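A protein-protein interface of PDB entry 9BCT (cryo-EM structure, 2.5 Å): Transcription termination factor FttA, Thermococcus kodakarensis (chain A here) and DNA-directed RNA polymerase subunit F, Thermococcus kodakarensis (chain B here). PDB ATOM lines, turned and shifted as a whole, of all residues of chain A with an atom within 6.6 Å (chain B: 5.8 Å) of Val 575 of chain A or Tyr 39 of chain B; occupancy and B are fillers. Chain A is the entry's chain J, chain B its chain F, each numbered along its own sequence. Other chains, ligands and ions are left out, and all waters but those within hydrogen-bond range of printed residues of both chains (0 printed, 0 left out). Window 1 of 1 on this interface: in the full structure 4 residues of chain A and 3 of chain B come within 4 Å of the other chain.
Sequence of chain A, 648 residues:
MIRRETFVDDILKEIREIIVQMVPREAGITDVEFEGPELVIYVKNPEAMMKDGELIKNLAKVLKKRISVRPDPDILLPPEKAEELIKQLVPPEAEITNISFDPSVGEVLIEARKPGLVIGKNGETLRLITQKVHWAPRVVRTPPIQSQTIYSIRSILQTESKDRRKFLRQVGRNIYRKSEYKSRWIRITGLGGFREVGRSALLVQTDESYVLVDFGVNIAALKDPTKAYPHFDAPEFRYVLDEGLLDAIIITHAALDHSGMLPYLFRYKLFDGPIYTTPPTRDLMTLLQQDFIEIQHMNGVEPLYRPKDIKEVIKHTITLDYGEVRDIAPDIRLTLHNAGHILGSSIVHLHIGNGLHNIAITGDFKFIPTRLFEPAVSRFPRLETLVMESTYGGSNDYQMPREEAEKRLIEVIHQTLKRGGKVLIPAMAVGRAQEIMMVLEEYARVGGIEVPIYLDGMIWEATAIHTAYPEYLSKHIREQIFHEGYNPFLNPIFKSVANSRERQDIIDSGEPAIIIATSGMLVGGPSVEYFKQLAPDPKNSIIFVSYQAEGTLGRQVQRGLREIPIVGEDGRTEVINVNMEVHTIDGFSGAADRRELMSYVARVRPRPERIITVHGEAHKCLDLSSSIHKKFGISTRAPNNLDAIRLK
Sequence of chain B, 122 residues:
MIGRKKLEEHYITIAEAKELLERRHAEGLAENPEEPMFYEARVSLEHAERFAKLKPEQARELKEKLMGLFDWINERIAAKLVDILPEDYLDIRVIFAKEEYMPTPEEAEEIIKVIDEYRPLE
OG1 of Thr 573 of chain A lies within hydrogen-bond range of OE2 of Glu 40 of chain B (2.7 Å). OE1 of Glu 563 of chain A is in salt-bridge range of NH1 of Arg 42 of chain B (3.3 Å).
OE2 of Glu 563 of chain A lies within hydrogen-bond range of ND2 of Asn 577 of chain A (2.7 Å).
Among the printed residues, merely in contact across the chains: Pro 565 of chain A with Tyr 39 of chain B (3.6 Å), Thr 573 of chain A with Tyr 39 of chain B (3.99 Å), Val 575 of chain A with Tyr 39 of chain B (3.6 Å) and Val 575 of chain A with Arg 42 of chain B (3.8 Å).
Val 575 of chain A touches just these residues of chain B: Tyr 39 (3.6 Å) and Arg 42 (3.8 Å). Printed residues of chain A within 4 Å of Tyr 39 of chain B: Pro 565 (3.6 Å), Thr 573 (3.99 Å) and Val 575 (3.6 Å). Printed residues of chain A within 4 Å of Glu 40 of chain B: Thr 573 (2.7 Å). Of the printed residues of chain A, Arg 42 of chain B touches Glu 563 (3.3 Å) and Val 575 (3.8 Å). Of the printed residues of chain B, Pro 565 of chain A touches Tyr 39 (3.6 Å). The nearest printed residue of chain B that does not touch Val 575 of chain A is Phe 38 of chain B (6.0 Å). The nearest printed residue of chain A that does not touch Tyr 39 of chain B is Glu 563 of chain A (5.1 Å). The nearest printed residue of chain A that does not touch Arg 42 of chain B is Asn 577 of chain A (6.4 Å).
Printed residues of chain B that touch a printed residue of chain A: Tyr 39, Glu 40 and Arg 42. Hydrophobic or aromatic side chains of chain B within 4 Å of the printed part of chain A: Tyr 39. Of the 9 printed residues of chain A, 4 touch a printed residue of chain B. Printed residues of chain A that touch a printed residue of chain B: Glu 563, Pro 565, Thr 573 and Val 575. Hydrophobic or aromatic side chains of chain A that line the printed part of chain B: Pro 565 and Val 575. Among the printed residues, Asp or Glu carboxylates within 4 Å of a Lys or Arg side-chain nitrogen of the other chain: Glu 563 of chain A with Arg 42 of chain B (3.3 Å).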
ATOM      1  N   GLU A 563     -11.163 -24.983 -15.784  1.00  0.00           N
ATOM      2  CA  GLU A 563     -10.435 -24.034 -14.944  1.00  0.00           C
ATOM      3  C   GLU A 563     -11.402 -22.938 -14.524  1.00  0.00           C
ATOM      4  O   GLU A 563     -11.752 -22.073 -15.335  1.00  0.00           O
ATOM      5  CB  GLU A 563      -9.231 -23.448 -15.681  1.00  0.00           C
ATOM      6  CG  GLU A 563      -7.964 -24.278 -15.557  1.00  0.00           C
ATOM      7  CD  GLU A 563      -6.706 -23.434 -15.613  1.00  0.00           C
ATOM      8  OE1 GLU A 563      -6.814 -22.221 -15.892  1.00  0.00           O
ATOM      9  OE2 GLU A 563      -5.609 -23.982 -15.376  1.00  0.00           O
ATOM     10  N   ILE A 564     -11.832 -22.971 -13.270  1.00  0.00           N
ATOM     11  CA  ILE A 564     -12.801 -22.018 -12.735  1.00  0.00           C
ATOM     12  C   ILE A 564     -12.047 -21.006 -11.880  1.00  0.00           C
ATOM     13  O   ILE A 564     -11.468 -21.393 -10.853  1.00  0.00           O
ATOM     14  CB  ILE A 564     -13.894 -22.722 -11.919  1.00  0.00           C
ATOM     15  CG1 ILE A 564     -14.813 -23.525 -12.840  1.00  0.00           C
ATOM     16  CG2 ILE A 564     -14.706 -21.705 -11.136  1.00  0.00           C
ATOM     17  CD1 ILE A 564     -15.116 -24.916 -12.332  1.00  0.00           C
ATOM     18  N   PRO A 565     -12.015 -19.726 -12.258  1.00  0.00           N
ATOM     19  CA  PRO A 565     -11.364 -18.709 -11.416  1.00  0.00           C
ATOM     20  C   PRO A 565     -12.288 -18.274 -10.287  1.00  0.00           C
ATOM     21  O   PRO A 565     -13.432 -17.876 -10.521  1.00  0.00           O
ATOM     22  CB  PRO A 565     -11.090 -17.564 -12.396  1.00  0.00           C
ATOM     23  CG  PRO A 565     -12.150 -17.703 -13.440  1.00  0.00           C
ATOM     24  CD  PRO A 565     -12.502 -19.168 -13.533  1.00  0.00           C
ATOM     25  N   ILE A 566     -11.792 -18.358  -9.053  1.00  0.00           N
ATOM     26  CA  ILE A 566     -12.555 -17.990  -7.870  1.00  0.00           C
ATOM     27  C   ILE A 566     -11.726 -17.035  -7.025  1.00  0.00           C
ATOM     28  O   ILE A 566     -10.512 -16.906  -7.206  1.00  0.00           O
ATOM     29  CB  ILE A 566     -12.973 -19.220  -7.032  1.00  0.00           C
ATOM     30  CG1 ILE A 566     -11.742 -19.917  -6.445  1.00  0.00           C
ATOM     31  CG2 ILE A 566     -13.812 -20.183  -7.859  1.00  0.00           C
ATOM     32  CD1 ILE A 566     -11.599 -19.764  -4.943  1.00  0.00           C
ATOM     33  N   THR A 573      -6.999 -13.896  -7.291  1.00  0.00           N
ATOM     34  CA  THR A 573      -7.746 -14.906  -8.026  1.00  0.00           C
ATOM     35  C   THR A 573      -6.948 -16.201  -8.103  1.00  0.00           C
ATOM     36  O   THR A 573      -5.837 -16.226  -8.641  1.00  0.00           O
ATOM     37  CB  THR A 573      -8.071 -14.400  -9.429  1.00  0.00           C
ATOM     38  OG1 THR A 573      -8.581 -13.063  -9.348  1.00  0.00           O
ATOM     39  CG2 THR A 573      -9.109 -15.292 -10.088  1.00  0.00           C
ATOM     40  N   GLU A 574      -7.515 -17.274  -7.561  1.00  0.00           N
ATOM     41  CA  GLU A 574      -6.930 -18.604  -7.641  1.00  0.00           C
ATOM     42  C   GLU A 574      -7.823 -19.477  -8.514  1.00  0.00           C
ATOM     43  O   GLU A 574      -9.054 -19.411  -8.418  1.00  0.00           O
ATOM     44  CB  GLU A 574      -6.730 -19.207  -6.243  1.00  0.00           C
ATOM     45  CG  GLU A 574      -7.880 -20.044  -5.695  1.00  0.00           C
ATOM     46  CD  GLU A 574      -7.445 -21.020  -4.620  1.00  0.00           C
ATOM     47  OE1 GLU A 574      -8.327 -21.655  -4.006  1.00  0.00           O
ATOM     48  OE2 GLU A 574      -6.226 -21.156  -4.389  1.00  0.00           O
ATOM     49  N   VAL A 575      -7.204 -20.235  -9.411  1.00  0.00           N
ATOM     50  CA  VAL A 575      -7.923 -21.079 -10.357  1.00  0.00           C
ATOM     51  C   VAL A 575      -8.047 -22.479  -9.775  1.00  0.00           C
ATOM     52  O   VAL A 575      -7.131 -22.969  -9.102  1.00  0.00           O
ATOM     53  CB  VAL A 575      -7.227 -21.102 -11.730  1.00  0.00           C
ATOM     54  CG1 VAL A 575      -7.230 -19.717 -12.338  1.00  0.00           C
ATOM     55  CG2 VAL A 575      -5.799 -21.612 -11.607  1.00  0.00           C
ATOM     56  N   ILE A 576      -9.192 -23.110 -10.008  1.00  0.00           N
ATOM     57  CA  ILE A 576      -9.392 -24.509  -9.656  1.00  0.00           C
ATOM     58  C   ILE A 576      -9.258 -25.320 -10.938  1.00  0.00           C
ATOM     59  O   ILE A 576     -10.090 -25.213 -11.843  1.00  0.00           O
ATOM     60  CB  ILE A 576     -10.753 -24.739  -8.988  1.00  0.00           C
ATOM     61  CG1 ILE A 576     -10.772 -24.142  -7.582  1.00  0.00           C
ATOM     62  CG2 ILE A 576     -11.071 -26.217  -8.922  1.00  0.00           C
ATOM     63  CD1 ILE A 576     -12.052 -23.418  -7.255  1.00  0.00           C
ATOM     64  N   ASN A 577      -8.204 -26.127 -11.023  1.00  0.00           N
ATOM     65  CA  ASN A 577      -7.977 -26.974 -12.190  1.00  0.00           C
ATOM     66  C   ASN A 577      -8.773 -28.257 -11.997  1.00  0.00           C
ATOM     67  O   ASN A 577      -8.345 -29.171 -11.289  1.00  0.00           O
ATOM     68  CB  ASN A 577      -6.491 -27.256 -12.371  1.00  0.00           C
ATOM     69  CG  ASN A 577      -5.689 -25.996 -12.632  1.00  0.00           C
ATOM     70  OD1 ASN A 577      -5.776 -25.025 -11.880  1.00  0.00           O
ATOM     71  ND2 ASN A 577      -4.901 -26.005 -13.701  1.00  0.00           N
ATOM     72  N   MET B  37       2.280 -16.751 -14.080  1.00  0.00           N
ATOM     73  CA  MET B  37       1.559 -15.674 -13.411  1.00  0.00           C
ATOM     74  C   MET B  37       0.227 -16.168 -12.863  1.00  0.00           C
ATOM     75  O   MET B  37      -0.051 -17.371 -12.876  1.00  0.00           O
ATOM     76  CB  MET B  37       1.321 -14.498 -14.362  1.00  0.00           C
ATOM     77  CG  MET B  37       2.448 -14.209 -15.340  1.00  0.00           C
ATOM     78  SD  MET B  37       2.176 -14.966 -16.954  1.00  0.00           S
ATOM     79  CE  MET B  37       1.280 -13.661 -17.792  1.00  0.00           C
ATOM     80  N   PHE B  38      -0.599 -15.245 -12.381  1.00  0.00           N
ATOM     81  CA  PHE B  38      -1.915 -15.576 -11.860  1.00  0.00           C
ATOM     82  C   PHE B  38      -2.919 -15.627 -13.010  1.00  0.00           C
ATOM     83  O   PHE B  38      -2.552 -15.593 -14.187  1.00  0.00           O
ATOM     84  CB  PHE B  38      -2.326 -14.579 -10.777  1.00  0.00           C
ATOM     85  CG  PHE B  38      -1.962 -13.154 -11.090  1.00  0.00           C
ATOM     86  CD1 PHE B  38      -2.815 -12.354 -11.831  1.00  0.00           C
ATOM     87  CD2 PHE B  38      -0.771 -12.612 -10.633  1.00  0.00           C
ATOM     88  CE1 PHE B  38      -2.484 -11.042 -12.116  1.00  0.00           C
ATOM     89  CE2 PHE B  38      -0.435 -11.303 -10.918  1.00  0.00           C
ATOM     90  CZ  PHE B  38      -1.293 -10.517 -11.660  1.00  0.00           C
ATOM     91  N   TYR B  39      -4.208 -15.716 -12.673  1.00  0.00           N
ATOM     92  CA  TYR B  39      -5.238 -15.833 -13.701  1.00  0.00           C
ATOM     93  C   TYR B  39      -5.374 -14.549 -14.510  1.00  0.00           C
ATOM     94  O   TYR B  39      -5.498 -14.594 -15.740  1.00  0.00           O
ATOM     95  CB  TYR B  39      -6.576 -16.203 -13.062  1.00  0.00           C
ATOM     96  CG  TYR B  39      -7.732 -16.246 -14.035  1.00  0.00           C
ATOM     97  CD1 TYR B  39      -7.870 -17.297 -14.933  1.00  0.00           C
ATOM     98  CD2 TYR B  39      -8.689 -15.240 -14.052  1.00  0.00           C
ATOM     99  CE1 TYR B  39      -8.926 -17.341 -15.823  1.00  0.00           C
ATOM    100  CE2 TYR B  39      -9.748 -15.276 -14.939  1.00  0.00           C
ATOM    101  CZ  TYR B  39      -9.862 -16.329 -15.821  1.00  0.00           C
ATOM    102  OH  TYR B  39     -10.915 -16.371 -16.706  1.00  0.00           O
ATOM    103  N   GLU B  40      -5.357 -13.395 -13.836  1.00  0.00           N
ATOM    104  CA  GLU B  40      -5.609 -12.131 -14.522  1.00  0.00           C
ATOM    105  C   GLU B  40      -4.504 -11.798 -15.516  1.00  0.00           C
ATOM    106  O   GLU B  40      -4.787 -11.367 -16.638  1.00  0.00           O
ATOM    107  CB  GLU B  40      -5.775 -11.006 -13.503  1.00  0.00           C
ATOM    108  CG  GLU B  40      -7.216 -10.753 -13.100  1.00  0.00           C
ATOM    109  CD  GLU B  40      -7.615 -11.527 -11.861  1.00  0.00           C
ATOM    110  OE1 GLU B  40      -6.735 -11.791 -11.016  1.00  0.00           O
ATOM    111  OE2 GLU B  40      -8.808 -11.873 -11.734  1.00  0.00           O
ATOM    112  N   ALA B  41      -3.240 -11.997 -15.132  1.00  0.00           N
ATOM    113  CA  ALA B  41      -2.138 -11.670 -16.032  1.00  0.00           C
ATOM    114  C   ALA B  41      -2.095 -12.612 -17.230  1.00  0.00           C
ATOM    115  O   ALA B  41      -1.849 -12.176 -18.361  1.00  0.00           O
ATOM    116  CB  ALA B  41      -0.813 -11.702 -15.273  1.00  0.00           C
ATOM    117  N   ARG B  42      -2.329 -13.907 -17.003  1.00  0.00           N
ATOM    118  CA  ARG B  42      -2.361 -14.861 -18.107  1.00  0.00           C
ATOM    119  C   ARG B  42      -3.517 -14.564 -19.056  1.00  0.00           C
ATOM    120  O   ARG B  42      -3.361 -14.630 -20.283  1.00  0.00           O
ATOM    121  CB  ARG B  42      -2.457 -16.286 -17.561  1.00  0.00           C
ATOM    122  CG  ARG B  42      -3.196 -17.266 -18.457  1.00  0.00           C
ATOM    123  CD  ARG B  42      -2.845 -18.702 -18.108  1.00  0.00           C
ATOM    124  NE  ARG B  42      -3.099 -18.997 -16.703  1.00  0.00           N
ATOM    125  CZ  ARG B  42      -4.279 -19.349 -16.212  1.00  0.00           C
ATOM    126  NH1 ARG B  42      -5.346 -19.461 -16.988  1.00  0.00           N
ATOM    127  NH2 ARG B  42      -4.394 -19.594 -14.910  1.00  0.00           N
ATOM    128  N   VAL B  43      -4.683 -14.221 -18.505  1.00  0.00           N
ATOM    129  CA  VAL B  43      -5.833 -13.880 -19.335  1.00  0.00           C
ATOM    130  C   VAL B  43      -5.568 -12.593 -20.111  1.00  0.00           C
ATOM    131  O   VAL B  43      -5.960 -12.465 -21.278  1.00  0.00           O
ATOM    132  CB  VAL B  43      -7.096 -13.794 -18.454  1.00  0.00           C
ATOM    133  CG1 VAL B  43      -7.969 -12.617 -18.836  1.00  0.00           C
ATOM    134  CG2 VAL B  43      -7.883 -15.094 -18.534  1.00  0.00           C
ATOM    135  N   SER B  44      -4.879 -11.632 -19.488  1.00  0.00           N
ATOM    136  CA  SER B  44      -4.502 -10.406 -20.183  1.00  0.00           C
ATOM    137  C   SER B  44      -3.550 -10.695 -21.335  1.00  0.00           C
ATOM    138  O   SER B  44      -3.686 -10.120 -22.420  1.00  0.00           O
ATOM    139  CB  SER B  44      -3.861  -9.427 -19.202  1.00  0.00           C
ATOM    140  OG  SER B  44      -4.815  -8.525 -18.682  1.00  0.00           O
